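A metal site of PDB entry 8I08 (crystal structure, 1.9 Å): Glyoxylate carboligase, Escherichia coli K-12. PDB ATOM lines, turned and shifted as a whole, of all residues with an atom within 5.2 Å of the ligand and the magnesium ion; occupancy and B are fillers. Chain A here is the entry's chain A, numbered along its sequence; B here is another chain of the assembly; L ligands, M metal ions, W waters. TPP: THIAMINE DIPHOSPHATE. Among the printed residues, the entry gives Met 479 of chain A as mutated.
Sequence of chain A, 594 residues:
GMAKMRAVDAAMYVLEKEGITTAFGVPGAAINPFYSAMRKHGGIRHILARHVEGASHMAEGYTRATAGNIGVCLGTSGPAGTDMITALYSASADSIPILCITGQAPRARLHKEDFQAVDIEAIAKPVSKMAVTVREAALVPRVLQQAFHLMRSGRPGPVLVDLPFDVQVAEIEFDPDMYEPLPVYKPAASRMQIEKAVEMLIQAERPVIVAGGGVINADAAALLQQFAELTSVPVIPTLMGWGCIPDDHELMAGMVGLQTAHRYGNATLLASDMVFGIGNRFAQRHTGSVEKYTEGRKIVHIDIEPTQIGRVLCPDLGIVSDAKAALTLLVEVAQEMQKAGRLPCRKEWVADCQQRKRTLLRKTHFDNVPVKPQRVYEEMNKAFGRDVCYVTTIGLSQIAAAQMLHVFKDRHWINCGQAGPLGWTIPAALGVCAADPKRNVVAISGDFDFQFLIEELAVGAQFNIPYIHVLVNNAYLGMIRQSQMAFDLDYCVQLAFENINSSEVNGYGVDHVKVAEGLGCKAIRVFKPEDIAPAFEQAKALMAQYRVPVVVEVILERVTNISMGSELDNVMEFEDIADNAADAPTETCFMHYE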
ATOM      1  N   ILE A 394      22.724 -32.000  10.168  1.00  0.00           N
ATOM      2  CA  ILE A 394      22.748 -31.946   8.707  1.00  0.00           C
ATOM      3  C   ILE A 394      23.071 -30.513   8.288  1.00  0.00           C
ATOM      4  O   ILE A 394      22.878 -29.574   9.054  1.00  0.00           O
ATOM      5  CB  ILE A 394      21.382 -32.423   8.130  1.00  0.00           C
ATOM      6  CG1 ILE A 394      21.501 -32.780   6.635  1.00  0.00           C
ATOM      7  CG2 ILE A 394      20.303 -31.375   8.395  1.00  0.00           C
ATOM      8  CD1 ILE A 394      20.281 -33.503   6.083  1.00  0.00           C
ATOM      9  N   GLY A 395      23.489 -30.357   7.045  1.00  0.00           N
ATOM     10  CA  GLY A 395      23.941 -29.090   6.486  1.00  0.00           C
ATOM     11  C   GLY A 395      25.374 -29.215   6.001  1.00  0.00           C
ATOM     12  O   GLY A 395      26.066 -30.195   6.284  1.00  0.00           O
ATOM     13  N   LEU A 396      25.818 -28.198   5.260  1.00  0.00           N
ATOM     14  CA  LEU A 396      27.228 -28.240   4.889  1.00  0.00           C
ATOM     15  C   LEU A 396      28.099 -28.233   6.146  1.00  0.00           C
ATOM     16  O   LEU A 396      29.182 -28.829   6.161  1.00  0.00           O
ATOM     17  CB  LEU A 396      27.597 -27.087   3.960  1.00  0.00           C
ATOM     18  CG  LEU A 396      26.849 -27.035   2.626  1.00  0.00           C
ATOM     19  CD1 LEU A 396      27.361 -25.873   1.731  1.00  0.00           C
ATOM     20  CD2 LEU A 396      26.927 -28.369   1.879  1.00  0.00           C
ATOM     21  N   SER A 397      27.605 -27.583   7.194  1.00  0.00           N
ATOM     22  CA  SER A 397      28.204 -27.661   8.518  1.00  0.00           C
ATOM     23  C   SER A 397      28.544 -29.100   8.888  1.00  0.00           C
ATOM     24  O   SER A 397      29.694 -29.400   9.267  1.00  0.00           O
ATOM     25  CB  SER A 397      27.206 -27.112   9.518  1.00  0.00           C
ATOM     26  OG  SER A 397      25.957 -27.803   9.345  1.00  0.00           O
ATOM     27  N   ALA A 419      17.554 -39.585   8.912  1.00  0.00           N
ATOM     28  CA  ALA A 419      16.434 -38.651   8.806  1.00  0.00           C
ATOM     29  C   ALA A 419      16.854 -37.187   8.852  1.00  0.00           C
ATOM     30  O   ALA A 419      16.154 -36.346   8.272  1.00  0.00           O
ATOM     31  CB  ALA A 419      15.385 -38.912   9.887  1.00  0.00           C
ATOM     32  N   GLY A 420      17.957 -36.849   9.528  1.00  0.00           N
ATOM     33  CA  GLY A 420      18.490 -35.500   9.547  1.00  0.00           C
ATOM     34  C   GLY A 420      17.498 -34.350   9.752  1.00  0.00           C
ATOM     35  O   GLY A 420      17.488 -33.388   8.988  1.00  0.00           O
ATOM     36  N   PRO A 421      16.664 -34.402  10.788  1.00  0.00           N
ATOM     37  CA  PRO A 421      15.716 -33.276  11.024  1.00  0.00           C
ATOM     38  C   PRO A 421      16.403 -32.057  11.616  1.00  0.00           C
ATOM     39  O   PRO A 421      16.885 -32.091  12.758  1.00  0.00           O
ATOM     40  CB  PRO A 421      14.693 -33.874  11.996  1.00  0.00           C
ATOM     41  CG  PRO A 421      15.460 -34.951  12.719  1.00  0.00           C
ATOM     42  CD  PRO A 421      16.496 -35.480  11.764  1.00  0.00           C
ATOM     43  N   LEU A 422      16.372 -30.955  10.891  1.00  0.00           N
ATOM     44  CA  LEU A 422      16.920 -29.701  11.418  1.00  0.00           C
ATOM     45  C   LEU A 422      16.276 -29.372  12.767  1.00  0.00           C
ATOM     46  O   LEU A 422      15.100 -29.633  12.967  1.00  0.00           O
ATOM     47  CB  LEU A 422      16.669 -28.562  10.432  1.00  0.00           C
ATOM     48  CG  LEU A 422      17.468 -28.603   9.134  1.00  0.00           C
ATOM     49  CD1 LEU A 422      16.831 -27.642   8.166  1.00  0.00           C
ATOM     50  CD2 LEU A 422      18.931 -28.194   9.402  1.00  0.00           C
ATOM     51  N   SER A 445      26.568 -27.052  14.482  1.00  0.00           N
ATOM     52  CA  SER A 445      25.375 -26.661  13.735  1.00  0.00           C
ATOM     53  C   SER A 445      25.742 -25.559  12.758  1.00  0.00           C
ATOM     54  O   SER A 445      26.606 -24.711  13.044  1.00  0.00           O
ATOM     55  CB  SER A 445      24.235 -26.068  14.611  1.00  0.00           C
ATOM     56  OG  SER A 445      23.551 -27.055  15.373  1.00  0.00           O
ATOM     57  N   GLY A 446      25.061 -25.574  11.593  1.00  0.00           N
ATOM     58  CA  GLY A 446      24.877 -24.365  10.805  1.00  0.00           C
ATOM     59  C   GLY A 446      23.826 -23.441  11.432  1.00  0.00           C
ATOM     60  O   GLY A 446      23.096 -23.804  12.371  1.00  0.00           O
ATOM     61  N   ASP A 447      23.763 -22.208  10.914  1.00  0.00           N
ATOM     62  CA  ASP A 447      22.874 -21.221  11.528  1.00  0.00           C
ATOM     63  C   ASP A 447      21.399 -21.619  11.425  1.00  0.00           C
ATOM     64  O   ASP A 447      20.641 -21.403  12.361  1.00  0.00           O
ATOM     65  CB  ASP A 447      23.117 -19.821  10.947  1.00  0.00           C
ATOM     66  CG  ASP A 447      23.259 -19.804   9.435  1.00  0.00           C
ATOM     67  OD1 ASP A 447      23.944 -20.668   8.845  1.00  0.00           O
ATOM     68  OD2 ASP A 447      22.698 -18.876   8.816  1.00  0.00           O
ATOM     69  N   PHE A 448      20.982 -22.248  10.321  1.00  0.00           N
ATOM     70  CA  PHE A 448      19.561 -22.582  10.174  1.00  0.00           C
ATOM     71  C   PHE A 448      19.160 -23.673  11.158  1.00  0.00           C
ATOM     72  O   PHE A 448      18.173 -23.541  11.899  1.00  0.00           O
ATOM     73  CB  PHE A 448      19.301 -23.019   8.729  1.00  0.00           C
ATOM     74  CG  PHE A 448      17.845 -22.964   8.278  1.00  0.00           C
ATOM     75  CD1 PHE A 448      17.063 -21.837   8.447  1.00  0.00           C
ATOM     76  CD2 PHE A 448      17.293 -24.047   7.580  1.00  0.00           C
ATOM     77  CE1 PHE A 448      15.761 -21.773   7.971  1.00  0.00           C
ATOM     78  CE2 PHE A 448      15.983 -24.007   7.087  1.00  0.00           C
ATOM     79  CZ  PHE A 448      15.210 -22.844   7.285  1.00  0.00           C
ATOM     80  N   ASP A 449      19.961 -24.743  11.229  1.00  0.00           N
ATOM     81  CA  ASP A 449      19.728 -25.816  12.186  1.00  0.00           C
ATOM     82  C   ASP A 449      19.651 -25.261  13.590  1.00  0.00           C
ATOM     83  O   ASP A 449      18.808 -25.683  14.395  1.00  0.00           O
ATOM     84  CB  ASP A 449      20.865 -26.844  12.065  1.00  0.00           C
ATOM     85  CG  ASP A 449      20.933 -27.850  13.231  1.00  0.00           C
ATOM     86  OD1 ASP A 449      19.872 -28.357  13.675  1.00  0.00           O
ATOM     87  OD2 ASP A 449      22.046 -28.164  13.701  1.00  0.00           O
ATOM     88  N   PHE A 450      20.538 -24.315  13.906  1.00  0.00           N
ATOM     89  CA  PHE A 450      20.621 -23.739  15.247  1.00  0.00           C
ATOM     90  C   PHE A 450      19.350 -22.985  15.594  1.00  0.00           C
ATOM     91  O   PHE A 450      18.926 -22.995  16.752  1.00  0.00           O
ATOM     92  CB  PHE A 450      21.840 -22.814  15.312  1.00  0.00           C
ATOM     93  CG  PHE A 450      22.225 -22.384  16.708  1.00  0.00           C
ATOM     94  CD1 PHE A 450      22.821 -23.271  17.584  1.00  0.00           C
ATOM     95  CD2 PHE A 450      22.016 -21.095  17.125  1.00  0.00           C
ATOM     96  CE1 PHE A 450      23.200 -22.865  18.856  1.00  0.00           C
ATOM     97  CE2 PHE A 450      22.386 -20.680  18.388  1.00  0.00           C
ATOM     98  CZ  PHE A 450      22.975 -21.560  19.256  1.00  0.00           C
ATOM     99  N   PHE A 452      16.135 -23.556  14.465  1.00  0.00           N
ATOM    100  CA  PHE A 452      14.866 -24.319  14.558  1.00  0.00           C
ATOM    101  C   PHE A 452      14.381 -24.488  16.002  1.00  0.00           C
ATOM    102  O   PHE A 452      13.235 -24.163  16.332  1.00  0.00           O
ATOM    103  CB  PHE A 452      15.016 -25.718  13.942  1.00  0.00           C
ATOM    104  CG  PHE A 452      14.520 -25.851  12.516  1.00  0.00           C
ATOM    105  CD1 PHE A 452      14.972 -24.997  11.511  1.00  0.00           C
ATOM    106  CD2 PHE A 452      13.640 -26.882  12.179  1.00  0.00           C
ATOM    107  CE1 PHE A 452      14.525 -25.157  10.202  1.00  0.00           C
ATOM    108  CE2 PHE A 452      13.195 -27.050  10.887  1.00  0.00           C
ATOM    109  CZ  PHE A 452      13.640 -26.184   9.887  1.00  0.00           C
ATOM    110  N   VAL A 472      28.521 -22.521  12.992  1.00  0.00           N
ATOM    111  CA  VAL A 472      29.230 -22.008  11.829  1.00  0.00           C
ATOM    112  C   VAL A 472      28.190 -21.301  10.962  1.00  0.00           C
ATOM    113  O   VAL A 472      27.261 -21.920  10.439  1.00  0.00           O
ATOM    114  CB  VAL A 472      30.029 -23.110  11.099  1.00  0.00           C
ATOM    115  CG1 VAL A 472      31.018 -23.757  12.073  1.00  0.00           C
ATOM    116  CG2 VAL A 472      29.178 -24.192  10.497  1.00  0.00           C
ATOM    117  N   ASN A 474      26.902 -18.971   7.974  1.00  0.00           N
ATOM    118  CA  ASN A 474      27.028 -18.367   6.660  1.00  0.00           C
ATOM    119  C   ASN A 474      25.800 -17.544   6.255  1.00  0.00           C
ATOM    120  O   ASN A 474      25.703 -17.128   5.098  1.00  0.00           O
ATOM    121  CB  ASN A 474      27.306 -19.452   5.600  1.00  0.00           C
ATOM    122  CG  ASN A 474      26.324 -20.618   5.685  1.00  0.00           C
ATOM    123  OD1 ASN A 474      25.196 -20.473   6.186  1.00  0.00           O
ATOM    124  ND2 ASN A 474      26.739 -21.787   5.176  1.00  0.00           N
ATOM    125  N   ALA A 475      24.857 -17.296   7.167  1.00  0.00           N
ATOM    126  CA  ALA A 475      23.606 -16.622   6.836  1.00  0.00           C
ATOM    127  C   ALA A 475      22.969 -17.234   5.583  1.00  0.00           C
ATOM    128  O   ALA A 475      22.459 -16.527   4.708  1.00  0.00           O
ATOM    129  CB  ALA A 475      23.800 -15.114   6.655  1.00  0.00           C
ATOM    130  N   TYR A 476      23.006 -18.565   5.493  1.00  0.00           N
ATOM    131  CA  TYR A 476      22.494 -19.271   4.316  1.00  0.00           C
ATOM    132  C   TYR A 476      21.936 -20.618   4.738  1.00  0.00           C
ATOM    133  O   TYR A 476      22.441 -21.241   5.676  1.00  0.00           O
ATOM    134  CB  TYR A 476      23.588 -19.566   3.305  1.00  0.00           C
ATOM    135  CG  TYR A 476      23.606 -18.802   1.987  1.00  0.00           C
ATOM    136  CD1 TYR A 476      22.765 -19.144   0.937  1.00  0.00           C
ATOM    137  CD2 TYR A 476      24.547 -17.805   1.771  1.00  0.00           C
ATOM    138  CE1 TYR A 476      22.819 -18.489  -0.261  1.00  0.00           C
ATOM    139  CE2 TYR A 476      24.615 -17.139   0.571  1.00  0.00           C
ATOM    140  CZ  TYR A 476      23.748 -17.484  -0.434  1.00  0.00           C
ATOM    141  OH  TYR A 476      23.822 -16.819  -1.642  1.00  0.00           O
ATOM    142  N   LEU A 477      20.938 -21.126   4.010  1.00  0.00           N
ATOM    143  CA  LEU A 477      20.762 -22.574   4.020  1.00  0.00           C
ATOM    144  C   LEU A 477      21.795 -23.092   3.019  1.00  0.00           C
ATOM    145  O   LEU A 477      21.511 -23.276   1.836  1.00  0.00           O
ATOM    146  CB  LEU A 477      19.349 -23.016   3.626  1.00  0.00           C
ATOM    147  CG  LEU A 477      18.070 -22.240   3.934  1.00  0.00           C
ATOM    148  CD1 LEU A 477      16.780 -23.094   3.765  1.00  0.00           C
ATOM    149  CD2 LEU A 477      18.093 -21.517   5.249  1.00  0.00           C
ATOM    150  N   GLY A 478      23.042 -23.309   3.499  1.00  0.00           N
ATOM    151  CA  GLY A 478      24.140 -23.516   2.572  1.00  0.00           C
ATOM    152  C   GLY A 478      24.001 -24.798   1.753  1.00  0.00           C
ATOM    153  O   GLY A 478      24.224 -24.794   0.536  1.00  0.00           O
ATOM    154  N   MET A 479      23.617 -25.904   2.400  1.00  0.00           N
ATOM    155  CA  MET A 479      23.461 -27.158   1.671  1.00  0.00           C
ATOM    156  C   MET A 479      22.489 -27.005   0.511  1.00  0.00           C
ATOM    157  O   MET A 479      22.664 -27.641  -0.529  1.00  0.00           O
ATOM    158  CB  MET A 479      22.980 -28.247   2.623  1.00  0.00           C
ATOM    159  CG  MET A 479      22.893 -29.671   2.067  1.00  0.00           C
ATOM    160  SD  MET A 479      22.735 -30.789   3.469  1.00  0.00           S
ATOM    161  CE  MET A 479      22.188 -32.301   2.660  1.00  0.00           C
ATOM    162  N   ILE A 480      21.483 -26.140   0.671  1.00  0.00           N
ATOM    163  CA  ILE A 480      20.421 -26.037  -0.316  1.00  0.00           C
ATOM    164  C   ILE A 480      20.824 -25.092  -1.424  1.00  0.00           C
ATOM    165  O   ILE A 480      20.507 -25.343  -2.584  1.00  0.00           O
ATOM    166  CB  ILE A 480      19.108 -25.591   0.345  1.00  0.00           C
ATOM    167  CG1 ILE A 480      18.845 -26.448   1.579  1.00  0.00           C
ATOM    168  CG2 ILE A 480      17.926 -25.668  -0.665  1.00  0.00           C
ATOM    169  CD1 ILE A 480      18.961 -27.928   1.341  1.00  0.00           C
ATOM    170  N   LEU A 495      19.478 -16.195   4.645  1.00  0.00           N
ATOM    171  CA  LEU A 495      18.965 -15.761   5.944  1.00  0.00           C
ATOM    172  C   LEU A 495      19.397 -14.354   6.326  1.00  0.00           C
ATOM    173  O   LEU A 495      19.020 -13.879   7.401  1.00  0.00           O
ATOM    174  CB  LEU A 495      19.390 -16.743   7.036  1.00  0.00           C
ATOM    175  CG  LEU A 495      18.737 -18.111   6.882  1.00  0.00           C
ATOM    176  CD1 LEU A 495      19.467 -19.124   7.725  1.00  0.00           C
ATOM    177  CD2 LEU A 495      17.241 -18.050   7.254  1.00  0.00           C
ATOM    178  N   VAL B  26      10.234 -24.128   3.553  1.00  0.00           N
ATOM    179  CA  VAL B  26      11.664 -24.358   3.738  1.00  0.00           C
ATOM    180  C   VAL B  26      12.097 -25.245   2.581  1.00  0.00           C
ATOM    181  O   VAL B  26      11.600 -26.376   2.474  1.00  0.00           O
ATOM    182  CB  VAL B  26      11.930 -25.040   5.082  1.00  0.00           C
ATOM    183  CG1 VAL B  26      13.436 -25.322   5.251  1.00  0.00           C
ATOM    184  CG2 VAL B  26      11.417 -24.190   6.214  1.00  0.00           C
ATOM    185  N   PRO B  27      12.977 -24.809   1.684  1.00  0.00           N
ATOM    186  CA  PRO B  27      13.377 -25.669   0.561  1.00  0.00           C
ATOM    187  C   PRO B  27      14.341 -26.776   1.005  1.00  0.00           C
ATOM    188  O   PRO B  27      14.884 -26.754   2.111  1.00  0.00           O
ATOM    189  CB  PRO B  27      14.049 -24.703  -0.414  1.00  0.00           C
ATOM    190  CG  PRO B  27      14.649 -23.658   0.498  1.00  0.00           C
ATOM    191  CD  PRO B  27      13.647 -23.484   1.614  1.00  0.00           C
ATOM    192  N   GLY B  28      14.520 -27.750   0.110  1.00  0.00           N
ATOM    193  CA  GLY B  28      15.550 -28.774   0.232  1.00  0.00           C
ATOM    194  C   GLY B  28      15.676 -29.524  -1.079  1.00  0.00           C
ATOM    195  O   GLY B  28      14.927 -29.274  -2.025  1.00  0.00           O
ATOM    196  N   VAL B  52      10.035 -25.738   9.850  1.00  0.00           N
ATOM    197  CA  VAL B  52       8.930 -26.180   8.999  1.00  0.00           C
ATOM    198  C   VAL B  52       7.625 -26.052   9.752  1.00  0.00           C
ATOM    199  O   VAL B  52       6.598 -25.673   9.185  1.00  0.00           O
ATOM    200  CB  VAL B  52       9.166 -27.624   8.510  1.00  0.00           C
ATOM    201  CG1 VAL B  52       7.876 -28.200   7.884  1.00  0.00           C
ATOM    202  CG2 VAL B  52      10.300 -27.660   7.518  1.00  0.00           C
ATOM    203  N   THR B  76      10.521 -30.165   2.122  1.00  0.00           N
ATOM    204  CA  THR B  76      11.229 -31.215   1.408  1.00  0.00           C
ATOM    205  C   THR B  76      10.732 -32.586   1.903  1.00  0.00           C
ATOM    206  O   THR B  76       9.646 -32.703   2.474  1.00  0.00           O
ATOM    207  CB  THR B  76      12.741 -30.978   1.518  1.00  0.00           C
ATOM    208  OG1 THR B  76      13.410 -31.783   0.550  1.00  0.00           O
ATOM    209  CG2 THR B  76      13.297 -31.305   2.930  1.00  0.00           C
ATOM    210  N   PRO B  79      11.829 -35.462   7.200  1.00  0.00           N
ATOM    211  CA  PRO B  79      11.336 -34.761   8.403  1.00  0.00           C
ATOM    212  C   PRO B  79      10.605 -33.448   8.108  1.00  0.00           C
ATOM    213  O   PRO B  79       9.985 -32.896   9.029  1.00  0.00           O
ATOM    214  CB  PRO B  79      12.618 -34.518   9.203  1.00  0.00           C
ATOM    215  CG  PRO B  79      13.670 -34.362   8.157  1.00  0.00           C
ATOM    216  CD  PRO B  79      13.291 -35.330   7.038  1.00  0.00           C
ATOM    217  N   ALA B  80      10.681 -32.916   6.897  1.00  0.00           N
ATOM    218  CA  ALA B  80       9.830 -31.771   6.590  1.00  0.00           C
ATOM    219  C   ALA B  80       8.362 -32.141   6.733  1.00  0.00           C
ATOM    220  O   ALA B  80       7.597 -31.432   7.373  1.00  0.00           O
ATOM    221  CB  ALA B  80      10.122 -31.243   5.180  1.00  0.00           C
ATOM    222  N   ASP B  83       7.190 -32.727  10.257  1.00  0.00           N
ATOM    223  CA  ASP B  83       7.068 -31.453  10.961  1.00  0.00           C
ATOM    224  C   ASP B  83       5.774 -30.711  10.620  1.00  0.00           C
ATOM    225  O   ASP B  83       5.539 -29.648  11.190  1.00  0.00           O
ATOM    226  CB  ASP B  83       8.237 -30.513  10.636  1.00  0.00           C
ATOM    227  CG  ASP B  83       9.483 -30.798  11.454  1.00  0.00           C
ATOM    228  OD1 ASP B  83       9.425 -31.576  12.438  1.00  0.00           O
ATOM    229  OD2 ASP B  83      10.532 -30.218  11.069  1.00  0.00           O
ATOM    230  N   GLN B 116      16.268 -39.957   3.803  1.00  0.00           N
ATOM    231  CA  GLN B 116      15.145 -39.068   4.152  1.00  0.00           C
ATOM    232  C   GLN B 116      13.871 -39.371   3.356  1.00  0.00           C
ATOM    233  O   GLN B 116      13.121 -38.451   3.030  1.00  0.00           O
ATOM    234  CB  GLN B 116      15.516 -37.587   3.974  1.00  0.00           C
ATOM    235  CG  GLN B 116      16.626 -37.109   4.903  1.00  0.00           C
ATOM    236  CD  GLN B 116      16.783 -35.567   4.956  1.00  0.00           C
ATOM    237  OE1 GLN B 116      16.881 -34.909   3.921  1.00  0.00           O
ATOM    238  NE2 GLN B 116      16.795 -35.017   6.168  1.00  0.00           N
HETATM  239  N1' TPP L   1      13.537 -29.236   6.598  1.00  0.00           N
HETATM  240  C2' TPP L   1      13.837 -30.038   7.639  1.00  0.00           C
HETATM  241  CM2 TPP L   1      12.867 -30.094   8.770  1.00  0.00           C
HETATM  242  N3' TPP L   1      14.942 -30.787   7.754  1.00  0.00           N
HETATM  243  C4' TPP L   1      15.828 -30.770   6.744  1.00  0.00           C
HETATM  244  N4' TPP L   1      16.919 -31.548   6.865  1.00  0.00           N
HETATM  245  C5' TPP L   1      15.621 -29.935   5.604  1.00  0.00           C
HETATM  246  C6' TPP L   1      14.452 -29.204   5.612  1.00  0.00           C
HETATM  247  C7' TPP L   1      16.582 -29.865   4.435  1.00  0.00           C
HETATM  248  N3  TPP L   1      17.895 -29.240   4.734  1.00  0.00           N
HETATM  249  C2  TPP L   1      19.034 -29.931   4.829  1.00  0.00           C
HETATM  250  S1  TPP L   1      20.371 -28.942   5.113  1.00  0.00           S
HETATM  251  C5  TPP L   1      19.377 -27.523   5.078  1.00  0.00           C
HETATM  252  C4  TPP L   1      18.066 -27.856   4.867  1.00  0.00           C
HETATM  253  CM4 TPP L   1      16.903 -26.923   4.762  1.00  0.00           C
HETATM  254  C6  TPP L   1      19.988 -26.185   5.348  1.00  0.00           C
HETATM  255  C7  TPP L   1      20.816 -26.188   6.609  1.00  0.00           C
HETATM  256  O7  TPP L   1      21.423 -24.893   6.815  1.00  0.00           O
HETATM  257  PA  TPP L   1      22.434 -24.594   7.987  1.00  0.00           P
HETATM  258  O1A TPP L   1      22.008 -25.363   9.220  1.00  0.00           O
HETATM  259  O2A TPP L   1      22.621 -23.124   8.037  1.00  0.00           O
HETATM  260  O3A TPP L   1      23.703 -25.246   7.375  1.00  0.00           O
HETATM  261  PB  TPP L   1      24.733 -24.907   6.222  1.00  0.00           P
HETATM  262  O1B TPP L   1      24.455 -23.496   5.804  1.00  0.00           O
HETATM  263  O2B TPP L   1      26.117 -25.162   6.861  1.00  0.00           O
HETATM  264  O3B TPP L   1      24.404 -25.886   5.095  1.00  0.00           O
HETATM  265 MG    MG M   1      23.958 -21.838   7.110  1.00  0.00          MG
HETATM  266  O   HOH W   1      28.926 -24.368   6.447  1.00  0.00           O
HETATM  267  O   HOH W   2      25.796 -22.668   8.045  1.00  0.00           O
HETATM  268  O   HOH W   3      11.653 -28.515   4.315  1.00  0.00           O
HETATM  269  O   HOH W   4      23.346 -27.300  10.123  1.00  0.00           O
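Ile 394 touches the ligand (CG2 to N4', 3.7 Å). Gly 395 touches the ligand (CA to O3B, 3.5 Å). Gly 446 touches the ligand. CE2 of Phe 452 touches CM2 of the ligand, 3.7 Å away. CB of Leu 477 touches C6 of the ligand, 3.7 Å away. CD1 of Ile 480 touches C4 of the ligand, at 3.6 Å. Val 26 of chain B touches the ligand (CG1 to CM4, 3.8 Å). Pro 27 of chain B touches the ligand (O to CM4, 3.3 Å). Val 52 of chain B touches the ligand (CG2 to N1', 3.7 Å). Thr 76 of chain B touches the ligand (CG2 to C6', 3.6 Å). Pro 79 of chain B touches the ligand (CG to N3', 3.8 Å). Asp 83 of chain B touches the ligand (OD2 to CM2, 3.3 Å). Gln 116 of chain B touches the ligand. Hydrophobic or aromatic side chains that line the ligand: Ile 394, Leu 396, Leu 422, Phe 448, Phe 452, Leu 477, Met 479, Ile 480, Val 26 of chain B, Val 52 of chain B and Pro 79 of chain B. The nearest printed residue that does not touch the ligand is Ala 80 of chain B (4.03 Å).
OD2 of Asp 447 sits close to N of Ala 475 (3.1 Å). SD of Met 479 lies close to N of Gly 395, at 3.7 Å. OG of Ser 397 is in hydrogen-bond range of N of Gly 446. The backbone carbonyl oxygen (O) of Gly 420 is in hydrogen-bond range of the side-chain amide nitrogen (NE2) of Gln 116 of chain B (3.3 Å). OD2 of Asp 449 is in hydrogen-bond range of OG of Ser 445 (2.5 Å). The side-chain amide nitrogen (NE2) of Gln 116 of chain B sits at hydrogen-bond distance from the backbone carbonyl oxygen (O) of Ala 419 (2.6 Å).
Three residues have an atom within 4 Å of the magnesium ion: Asp 447, Asn 474 and Tyr 476. The nearest printed residue that does not touch the magnesium ion is Gly 478 (4.01 Å).
An oxygen (O2A) of the ligand sits close to the backbone NH of Asp 447 (3.2 Å). O3B of the ligand sits at hydrogen-bond distance from N of Gly 478, 3.3 Å away. The backbone NH (N) of Leu 396 is in hydrogen-bond range of an oxygen (O3B) of the ligand (2.7 Å). An oxygen (O3B) of the ligand lies within hydrogen-bond range of the backbone NH (N) of Met 479 (2.8 Å). The backbone NH of Ser 397 is in hydrogen-bond range of an oxygen (O2B) of the ligand, 2.9 Å away. The backbone carbonyl oxygen of Gly 420 is in hydrogen-bond range of a nitrogen (N4') of the ligand. An oxygen (O1A) of the ligand lies within hydrogen-bond range of the backbone NH (N) of Asp 449 (2.9 Å). O1A of the ligand sits at hydrogen-bond distance from N of Phe 448, at 3.5 Å. The backbone NH (N) of Leu 422 is in hydrogen-bond range of a nitrogen (N3') of the ligand, at 3.5 Å.
The magnesium ion is bound by OD1 of Asn 474, 2.1 Å away. O2A of the ligand binds the magnesium ion, at 2.1 Å. OD1 of Asp 447 is bound to the magnesium ion (2.1 Å). The magnesium ion is bound by an oxygen (O1B) of the ligand (2.2 Å). The magnesium ion is bound by O of Tyr 476. Water W2 is bound to the magnesium ion (2.2 Å). The magnesium ion has six donor atoms within binding distance.
Water W2 lies within hydrogen-bond range of O2B of the ligand (2.8 Å), O of Val 472 (2.9 Å) and ND2 of Asn 474 (3.1 Å). Water W4 lies within hydrogen-bond range of an oxygen (O1A) of the ligand, the backbone carbonyl oxygen (O) of Ile 394, the side-chain hydroxyl (OG) of Ser 397 and the backbone NH (N) of Gly 446. Water W3 lies within hydrogen-bond range of the backbone carbonyl oxygen of Val 26 of chain B, the backbone NH of Thr 76 of chain B and a nitrogen (N1') of the ligand.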
